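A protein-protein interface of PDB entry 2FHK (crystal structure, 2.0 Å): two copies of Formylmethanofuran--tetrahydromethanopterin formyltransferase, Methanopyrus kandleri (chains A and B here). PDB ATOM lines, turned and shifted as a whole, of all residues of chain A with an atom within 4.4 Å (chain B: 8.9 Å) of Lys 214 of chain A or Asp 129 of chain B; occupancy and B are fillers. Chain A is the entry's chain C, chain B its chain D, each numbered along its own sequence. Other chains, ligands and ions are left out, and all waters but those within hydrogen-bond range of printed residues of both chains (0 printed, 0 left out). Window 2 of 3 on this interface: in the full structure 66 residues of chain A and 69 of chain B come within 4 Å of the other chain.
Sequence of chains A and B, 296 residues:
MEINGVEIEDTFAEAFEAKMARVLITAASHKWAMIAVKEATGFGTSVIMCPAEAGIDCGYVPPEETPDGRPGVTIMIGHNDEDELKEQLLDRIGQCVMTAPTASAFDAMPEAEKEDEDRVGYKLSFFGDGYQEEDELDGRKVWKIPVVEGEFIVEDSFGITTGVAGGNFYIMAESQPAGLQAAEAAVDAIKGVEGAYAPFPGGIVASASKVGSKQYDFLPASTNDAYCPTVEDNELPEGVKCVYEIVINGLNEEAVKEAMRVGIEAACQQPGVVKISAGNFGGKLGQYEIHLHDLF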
ATOM      1  N   LYS A 210      27.030  29.401  21.546  1.00  0.00           N
ATOM      2  CA  LYS A 210      27.965  29.579  22.651  1.00  0.00           C
ATOM      3  C   LYS A 210      29.356  29.127  22.205  1.00  0.00           C
ATOM      4  O   LYS A 210      29.496  28.435  21.197  1.00  0.00           O
ATOM      5  CB  LYS A 210      27.513  28.773  23.876  1.00  0.00           C
ATOM      6  CG  LYS A 210      27.623  27.253  23.731  1.00  0.00           C
ATOM      7  CD  LYS A 210      26.966  26.537  24.894  1.00  0.00           C
ATOM      8  CE  LYS A 210      27.222  25.033  24.836  1.00  0.00           C
ATOM      9  NZ  LYS A 210      26.254  24.319  23.944  1.00  0.00           N
ATOM     10  N   SER A 213      31.556  23.467  22.955  1.00  0.00           N
ATOM     11  CA  SER A 213      30.472  22.503  23.095  1.00  0.00           C
ATOM     12  C   SER A 213      30.679  21.677  24.352  1.00  0.00           C
ATOM     13  O   SER A 213      31.811  21.316  24.685  1.00  0.00           O
ATOM     14  CB  SER A 213      30.417  21.579  21.872  1.00  0.00           C
ATOM     15  OG  SER A 213      29.749  20.362  22.170  1.00  0.00           O
ATOM     16  N   LYS A 214      29.579  21.370  25.034  1.00  0.00           N
ATOM     17  CA  LYS A 214      29.607  20.516  26.219  1.00  0.00           C
ATOM     18  C   LYS A 214      29.924  19.057  25.874  1.00  0.00           C
ATOM     19  O   LYS A 214      30.518  18.332  26.681  1.00  0.00           O
ATOM     20  CB  LYS A 214      28.277  20.593  26.970  1.00  0.00           C
ATOM     21  CG  LYS A 214      28.062  21.892  27.747  1.00  0.00           C
ATOM     22  CD  LYS A 214      26.852  21.808  28.691  1.00  0.00           C
ATOM     23  CE  LYS A 214      25.525  22.179  28.011  1.00  0.00           C
ATOM     24  NZ  LYS A 214      25.002  21.112  27.105  1.00  0.00           N
ATOM     25  N   GLN A 215      29.541  18.638  24.669  1.00  0.00           N
ATOM     26  CA  GLN A 215      29.625  17.230  24.293  1.00  0.00           C
ATOM     27  C   GLN A 215      30.693  16.884  23.250  1.00  0.00           C
ATOM     28  O   GLN A 215      31.205  15.764  23.249  1.00  0.00           O
ATOM     29  CB  GLN A 215      28.254  16.728  23.833  1.00  0.00           C
ATOM     30  CG  GLN A 215      27.963  15.292  24.249  1.00  0.00           C
ATOM     31  CD  GLN A 215      27.801  15.135  25.753  1.00  0.00           C
ATOM     32  OE1 GLN A 215      27.347  16.050  26.448  1.00  0.00           O
ATOM     33  NE2 GLN A 215      28.163  13.960  26.263  1.00  0.00           N
ATOM     34  N   TYR A 216      31.021  17.831  22.372  1.00  0.00           N
ATOM     35  CA  TYR A 216      31.877  17.543  21.215  1.00  0.00           C
ATOM     36  C   TYR A 216      33.117  18.435  21.147  1.00  0.00           C
ATOM     37  O   TYR A 216      33.021  19.643  20.920  1.00  0.00           O
ATOM     38  CB  TYR A 216      31.068  17.614  19.909  1.00  0.00           C
ATOM     39  CG  TYR A 216      29.740  16.879  19.984  1.00  0.00           C
ATOM     40  CD1 TYR A 216      28.536  17.579  19.969  1.00  0.00           C
ATOM     41  CD2 TYR A 216      29.692  15.488  20.100  1.00  0.00           C
ATOM     42  CE1 TYR A 216      27.314  16.913  20.057  1.00  0.00           C
ATOM     43  CE2 TYR A 216      28.477  14.816  20.191  1.00  0.00           C
ATOM     44  CZ  TYR A 216      27.293  15.536  20.169  1.00  0.00           C
ATOM     45  OH  TYR A 216      26.089  14.876  20.247  1.00  0.00           O
ATOM     46  N   SER A 222      28.617  25.836  19.396  1.00  0.00           N
ATOM     47  CA  SER A 222      27.430  24.984  19.384  1.00  0.00           C
ATOM     48  C   SER A 222      26.204  25.801  19.787  1.00  0.00           C
ATOM     49  O   SER A 222      26.300  27.001  20.026  1.00  0.00           O
ATOM     50  CB  SER A 222      27.604  23.797  20.323  1.00  0.00           C
ATOM     51  OG  SER A 222      27.766  24.240  21.651  1.00  0.00           O
ATOM     52  N   ASP A 225      21.927  26.467  24.221  1.00  0.00           N
ATOM     53  CA  ASP A 225      20.819  25.625  24.711  1.00  0.00           C
ATOM     54  C   ASP A 225      19.933  26.243  25.798  1.00  0.00           C
ATOM     55  O   ASP A 225      18.761  25.897  25.917  1.00  0.00           O
ATOM     56  CB  ASP A 225      21.325  24.238  25.153  1.00  0.00           C
ATOM     57  CG  ASP A 225      22.615  24.301  25.969  1.00  0.00           C
ATOM     58  OD1 ASP A 225      23.646  24.779  25.441  1.00  0.00           O
ATOM     59  OD2 ASP A 225      22.603  23.848  27.136  1.00  0.00           O
ATOM     60  N   LEU B 124      25.761  18.599  10.663  1.00  0.00           N
ATOM     61  CA  LEU B 124      25.217  19.787  11.320  1.00  0.00           C
ATOM     62  C   LEU B 124      24.507  19.487  12.633  1.00  0.00           C
ATOM     63  O   LEU B 124      24.449  20.355  13.500  1.00  0.00           O
ATOM     64  CB  LEU B 124      24.254  20.534  10.390  1.00  0.00           C
ATOM     65  CG  LEU B 124      24.793  21.236   9.139  1.00  0.00           C
ATOM     66  CD1 LEU B 124      23.634  21.806   8.325  1.00  0.00           C
ATOM     67  CD2 LEU B 124      25.776  22.331   9.496  1.00  0.00           C
ATOM     68  N   SER B 125      23.980  18.271  12.779  1.00  0.00           N
ATOM     69  CA  SER B 125      23.160  17.895  13.944  1.00  0.00           C
ATOM     70  C   SER B 125      23.880  18.046  15.287  1.00  0.00           C
ATOM     71  O   SER B 125      23.239  18.284  16.307  1.00  0.00           O
ATOM     72  CB  SER B 125      22.599  16.477  13.795  1.00  0.00           C
ATOM     73  OG  SER B 125      23.620  15.494  13.867  1.00  0.00           O
ATOM     74  N   PHE B 126      25.206  17.925  15.267  1.00  0.00           N
ATOM     75  CA  PHE B 126      26.030  17.994  16.478  1.00  0.00           C
ATOM     76  C   PHE B 126      26.007  19.375  17.143  1.00  0.00           C
ATOM     77  O   PHE B 126      26.312  19.511  18.330  1.00  0.00           O
ATOM     78  CB  PHE B 126      27.463  17.555  16.164  1.00  0.00           C
ATOM     79  CG  PHE B 126      27.582  16.096  15.810  1.00  0.00           C
ATOM     80  CD1 PHE B 126      27.502  15.680  14.485  1.00  0.00           C
ATOM     81  CD2 PHE B 126      27.757  15.138  16.804  1.00  0.00           C
ATOM     82  CE1 PHE B 126      27.604  14.333  14.157  1.00  0.00           C
ATOM     83  CE2 PHE B 126      27.863  13.784  16.487  1.00  0.00           C
ATOM     84  CZ  PHE B 126      27.788  13.383  15.161  1.00  0.00           C
ATOM     85  N   PHE B 127      25.638  20.389  16.364  1.00  0.00           N
ATOM     86  CA  PHE B 127      25.356  21.729  16.878  1.00  0.00           C
ATOM     87  C   PHE B 127      24.313  21.714  17.997  1.00  0.00           C
ATOM     88  O   PHE B 127      24.363  22.551  18.891  1.00  0.00           O
ATOM     89  CB  PHE B 127      24.895  22.630  15.732  1.00  0.00           C
ATOM     90  CG  PHE B 127      24.808  24.089  16.087  1.00  0.00           C
ATOM     91  CD1 PHE B 127      23.578  24.680  16.363  1.00  0.00           C
ATOM     92  CD2 PHE B 127      25.951  24.883  16.115  1.00  0.00           C
ATOM     93  CE1 PHE B 127      23.485  26.036  16.672  1.00  0.00           C
ATOM     94  CE2 PHE B 127      25.867  26.238  16.432  1.00  0.00           C
ATOM     95  CZ  PHE B 127      24.625  26.813  16.712  1.00  0.00           C
ATOM     96  N   GLY B 128      23.391  20.754  17.950  1.00  0.00           N
ATOM     97  CA  GLY B 128      22.366  20.576  18.985  1.00  0.00           C
ATOM     98  C   GLY B 128      22.884  20.129  20.350  1.00  0.00           C
ATOM     99  O   GLY B 128      22.117  20.050  21.312  1.00  0.00           O
ATOM    100  N   ASP B 129      24.179  19.819  20.423  1.00  0.00           N
ATOM    101  CA  ASP B 129      24.875  19.497  21.682  1.00  0.00           C
ATOM    102  C   ASP B 129      24.206  18.396  22.519  1.00  0.00           C
ATOM    103  O   ASP B 129      24.243  18.441  23.753  1.00  0.00           O
ATOM    104  CB  ASP B 129      25.075  20.776  22.523  1.00  0.00           C
ATOM    105  CG  ASP B 129      26.308  20.711  23.429  1.00  0.00           C
ATOM    106  OD1 ASP B 129      27.159  19.804  23.263  1.00  0.00           O
ATOM    107  OD2 ASP B 129      26.436  21.593  24.310  1.00  0.00           O
ATOM    108  N   GLY B 130      23.611  17.414  21.845  1.00  0.00           N
ATOM    109  CA  GLY B 130      22.979  16.283  22.523  1.00  0.00           C
ATOM    110  C   GLY B 130      21.471  16.283  22.428  1.00  0.00           C
ATOM    111  O   GLY B 130      20.850  15.234  22.547  1.00  0.00           O
ATOM    112  N   TYR B 131      20.889  17.462  22.205  1.00  0.00           N
ATOM    113  CA  TYR B 131      19.434  17.631  22.161  1.00  0.00           C
ATOM    114  C   TYR B 131      18.840  17.444  20.767  1.00  0.00           C
ATOM    115  O   TYR B 131      17.619  17.402  20.614  1.00  0.00           O
ATOM    116  CB  TYR B 131      19.032  19.005  22.715  1.00  0.00           C
ATOM    117  CG  TYR B 131      19.492  19.276  24.129  1.00  0.00           C
ATOM    118  CD1 TYR B 131      20.702  19.925  24.374  1.00  0.00           C
ATOM    119  CD2 TYR B 131      18.711  18.894  25.224  1.00  0.00           C
ATOM    120  CE1 TYR B 131      21.128  20.179  25.672  1.00  0.00           C
ATOM    121  CE2 TYR B 131      19.128  19.145  26.524  1.00  0.00           C
ATOM    122  CZ  TYR B 131      20.338  19.786  26.740  1.00  0.00           C
ATOM    123  OH  TYR B 131      20.757  20.038  28.026  1.00  0.00           O
ATOM    124  N   GLN B 132      19.700  17.343  19.750  1.00  0.00           N
ATOM    125  CA  GLN B 132      19.238  17.068  18.383  1.00  0.00           C
ATOM    126  C   GLN B 132      18.536  15.713  18.303  1.00  0.00           C
ATOM    127  O   GLN B 132      18.814  14.803  19.092  1.00  0.00           O
ATOM    128  CB  GLN B 132      20.386  17.133  17.371  1.00  0.00           C
ATOM    129  CG  GLN B 132      21.361  15.951  17.422  1.00  0.00           C
ATOM    130  CD  GLN B 132      22.493  16.155  18.409  1.00  0.00           C
ATOM    131  OE1 GLN B 132      22.381  16.949  19.342  1.00  0.00           O
ATOM    132  NE2 GLN B 132      23.599  15.445  18.203  1.00  0.00           N
ATOM    133  N   GLU B 133      17.639  15.590  17.334  1.00  0.00           N
ATOM    134  CA  GLU B 133      16.733  14.465  17.263  1.00  0.00           C
ATOM    135  C   GLU B 133      16.433  14.161  15.799  1.00  0.00           C
ATOM    136  O   GLU B 133      16.049  15.052  15.038  1.00  0.00           O
ATOM    137  CB  GLU B 133      15.459  14.803  18.055  1.00  0.00           C
ATOM    138  CG  GLU B 133      14.187  14.049  17.683  1.00  0.00           C
ATOM    139  CD  GLU B 133      13.014  14.458  18.557  1.00  0.00           C
ATOM    140  OE1 GLU B 133      11.858  14.326  18.100  1.00  0.00           O
ATOM    141  OE2 GLU B 133      13.245  14.914  19.701  1.00  0.00           O
ATOM    142  N   LYS B 144      16.257  17.378  13.574  1.00  0.00           N
ATOM    143  CA  LYS B 144      15.651  18.536  14.214  1.00  0.00           C
ATOM    144  C   LYS B 144      16.645  19.073  15.236  1.00  0.00           C
ATOM    145  O   LYS B 144      16.852  18.470  16.298  1.00  0.00           O
ATOM    146  CB  LYS B 144      14.323  18.165  14.869  1.00  0.00           C
ATOM    147  CG  LYS B 144      13.324  17.488  13.929  1.00  0.00           C
ATOM    148  CD  LYS B 144      11.925  17.416  14.540  1.00  0.00           C
ATOM    149  CE  LYS B 144      11.876  16.462  15.735  1.00  0.00           C
ATOM    150  NZ  LYS B 144      10.489  16.269  16.259  1.00  0.00           N
ATOM    151  N   ILE B 145      17.285  20.187  14.886  1.00  0.00           N
ATOM    152  CA  ILE B 145      18.330  20.784  15.706  1.00  0.00           C
ATOM    153  C   ILE B 145      17.754  21.947  16.511  1.00  0.00           C
ATOM    154  O   ILE B 145      17.237  22.908  15.923  1.00  0.00           O
ATOM    155  CB  ILE B 145      19.513  21.284  14.838  1.00  0.00           C
ATOM    156  CG1 ILE B 145      20.055  20.153  13.958  1.00  0.00           C
ATOM    157  CG2 ILE B 145      20.613  21.880  15.706  1.00  0.00           C
ATOM    158  CD1 ILE B 145      20.915  20.639  12.797  1.00  0.00           C
ATOM    159  N   PRO B 146      17.846  21.868  17.855  1.00  0.00           N
ATOM    160  CA  PRO B 146      17.286  22.907  18.713  1.00  0.00           C
ATOM    161  C   PRO B 146      18.073  24.192  18.544  1.00  0.00           C
ATOM    162  O   PRO B 146      19.301  24.192  18.639  1.00  0.00           O
ATOM    163  CB  PRO B 146      17.486  22.354  20.133  1.00  0.00           C
ATOM    164  CG  PRO B 146      17.822  20.931  19.968  1.00  0.00           C
ATOM    165  CD  PRO B 146      18.501  20.814  18.647  1.00  0.00           C
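N of Gly 130 of chain B sits at hydrogen-bond distance from OE1 of Gln 132 of chain B, at 2.8 Å. The side-chain amino group of Lys 210 of chain A lies within salt-bridge range of the side-chain carboxylate of Asp 225 of chain A (3.0 Å). OG of Ser 213 of chain A is in hydrogen-bond range of N of Tyr 216 of chain A (2.8 Å). OG of Ser 213 of chain A sits at hydrogen-bond distance from N of Gln 215 of chain A, at 3.0 Å. The side-chain amino group (NZ) of Lys 210 of chain A sits at hydrogen-bond distance from the side-chain hydroxyl (OG) of Ser 222 of chain A (2.7 Å). The side-chain amino group of Lys 214 of chain A lies within salt-bridge range of the side-chain carboxylate of Asp 225 of chain A, at 3.6 Å.
Hydrophobic or aromatic side chains of chain B that line the printed part of chain A: Phe 126 and Phe 127.
Lys 214 of chain A touches just one residue of chain B: Asp 129. Printed residues of chain A within 4 Å of Phe 126 of chain B: Tyr 216 (3.3 Å). Of the printed residues of chain A, Asp 129 of chain B touches Lys 210 (2.8 Å), Ser 213 (2.9 Å), Lys 214 (3.2 Å), Gln 215 (3.0 Å), Tyr 216 (3.9 Å) and Ser 222 (3.98 Å). Printed residues of chain A within 4 Å of Gln 132 of chain B: Tyr 216.
Among the printed residues, pairs that only touch across the chains: Tyr 216 of chain A with Phe 126 of chain B (3.3 Å), Ser 222 of chain A with Phe 127 of chain B (3.4 Å), Tyr 216 of chain A with Gly 130 of chain B (3.9 Å), Tyr 216 of chain A with Asp 129 of chain B (3.9 Å) and Ser 222 of chain A with Asp 129 of chain B (3.98 Å).
The side-chain amino group (NZ) of Lys 210 of chain A is in salt-bridge range of the side-chain carboxylate (OD2) of Asp 129 of chain B, 2.8 Å away. The side-chain hydroxyl (OG) of Ser 213 of chain A lies within hydrogen-bond range of the side-chain carboxylate (OD1) of Asp 129 of chain B. The backbone NH of Gln 215 of chain A lies within hydrogen-bond range of the side-chain carboxylate of Asp 129 of chain B (3.0 Å). The side-chain hydroxyl (OH) of Tyr 216 of chain A lies within hydrogen-bond range of the side-chain amide nitrogen (NE2) of Gln 132 of chain B, at 3.3 Å. NZ of Lys 214 of chain A is in salt-bridge range of OD2 of Asp 129 of chain B (3.2 Å).
No position is printed for both chains. Of the 10 pairs that touch across the chains among the printed residues, none has its exchanged pair printed and touching as well.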
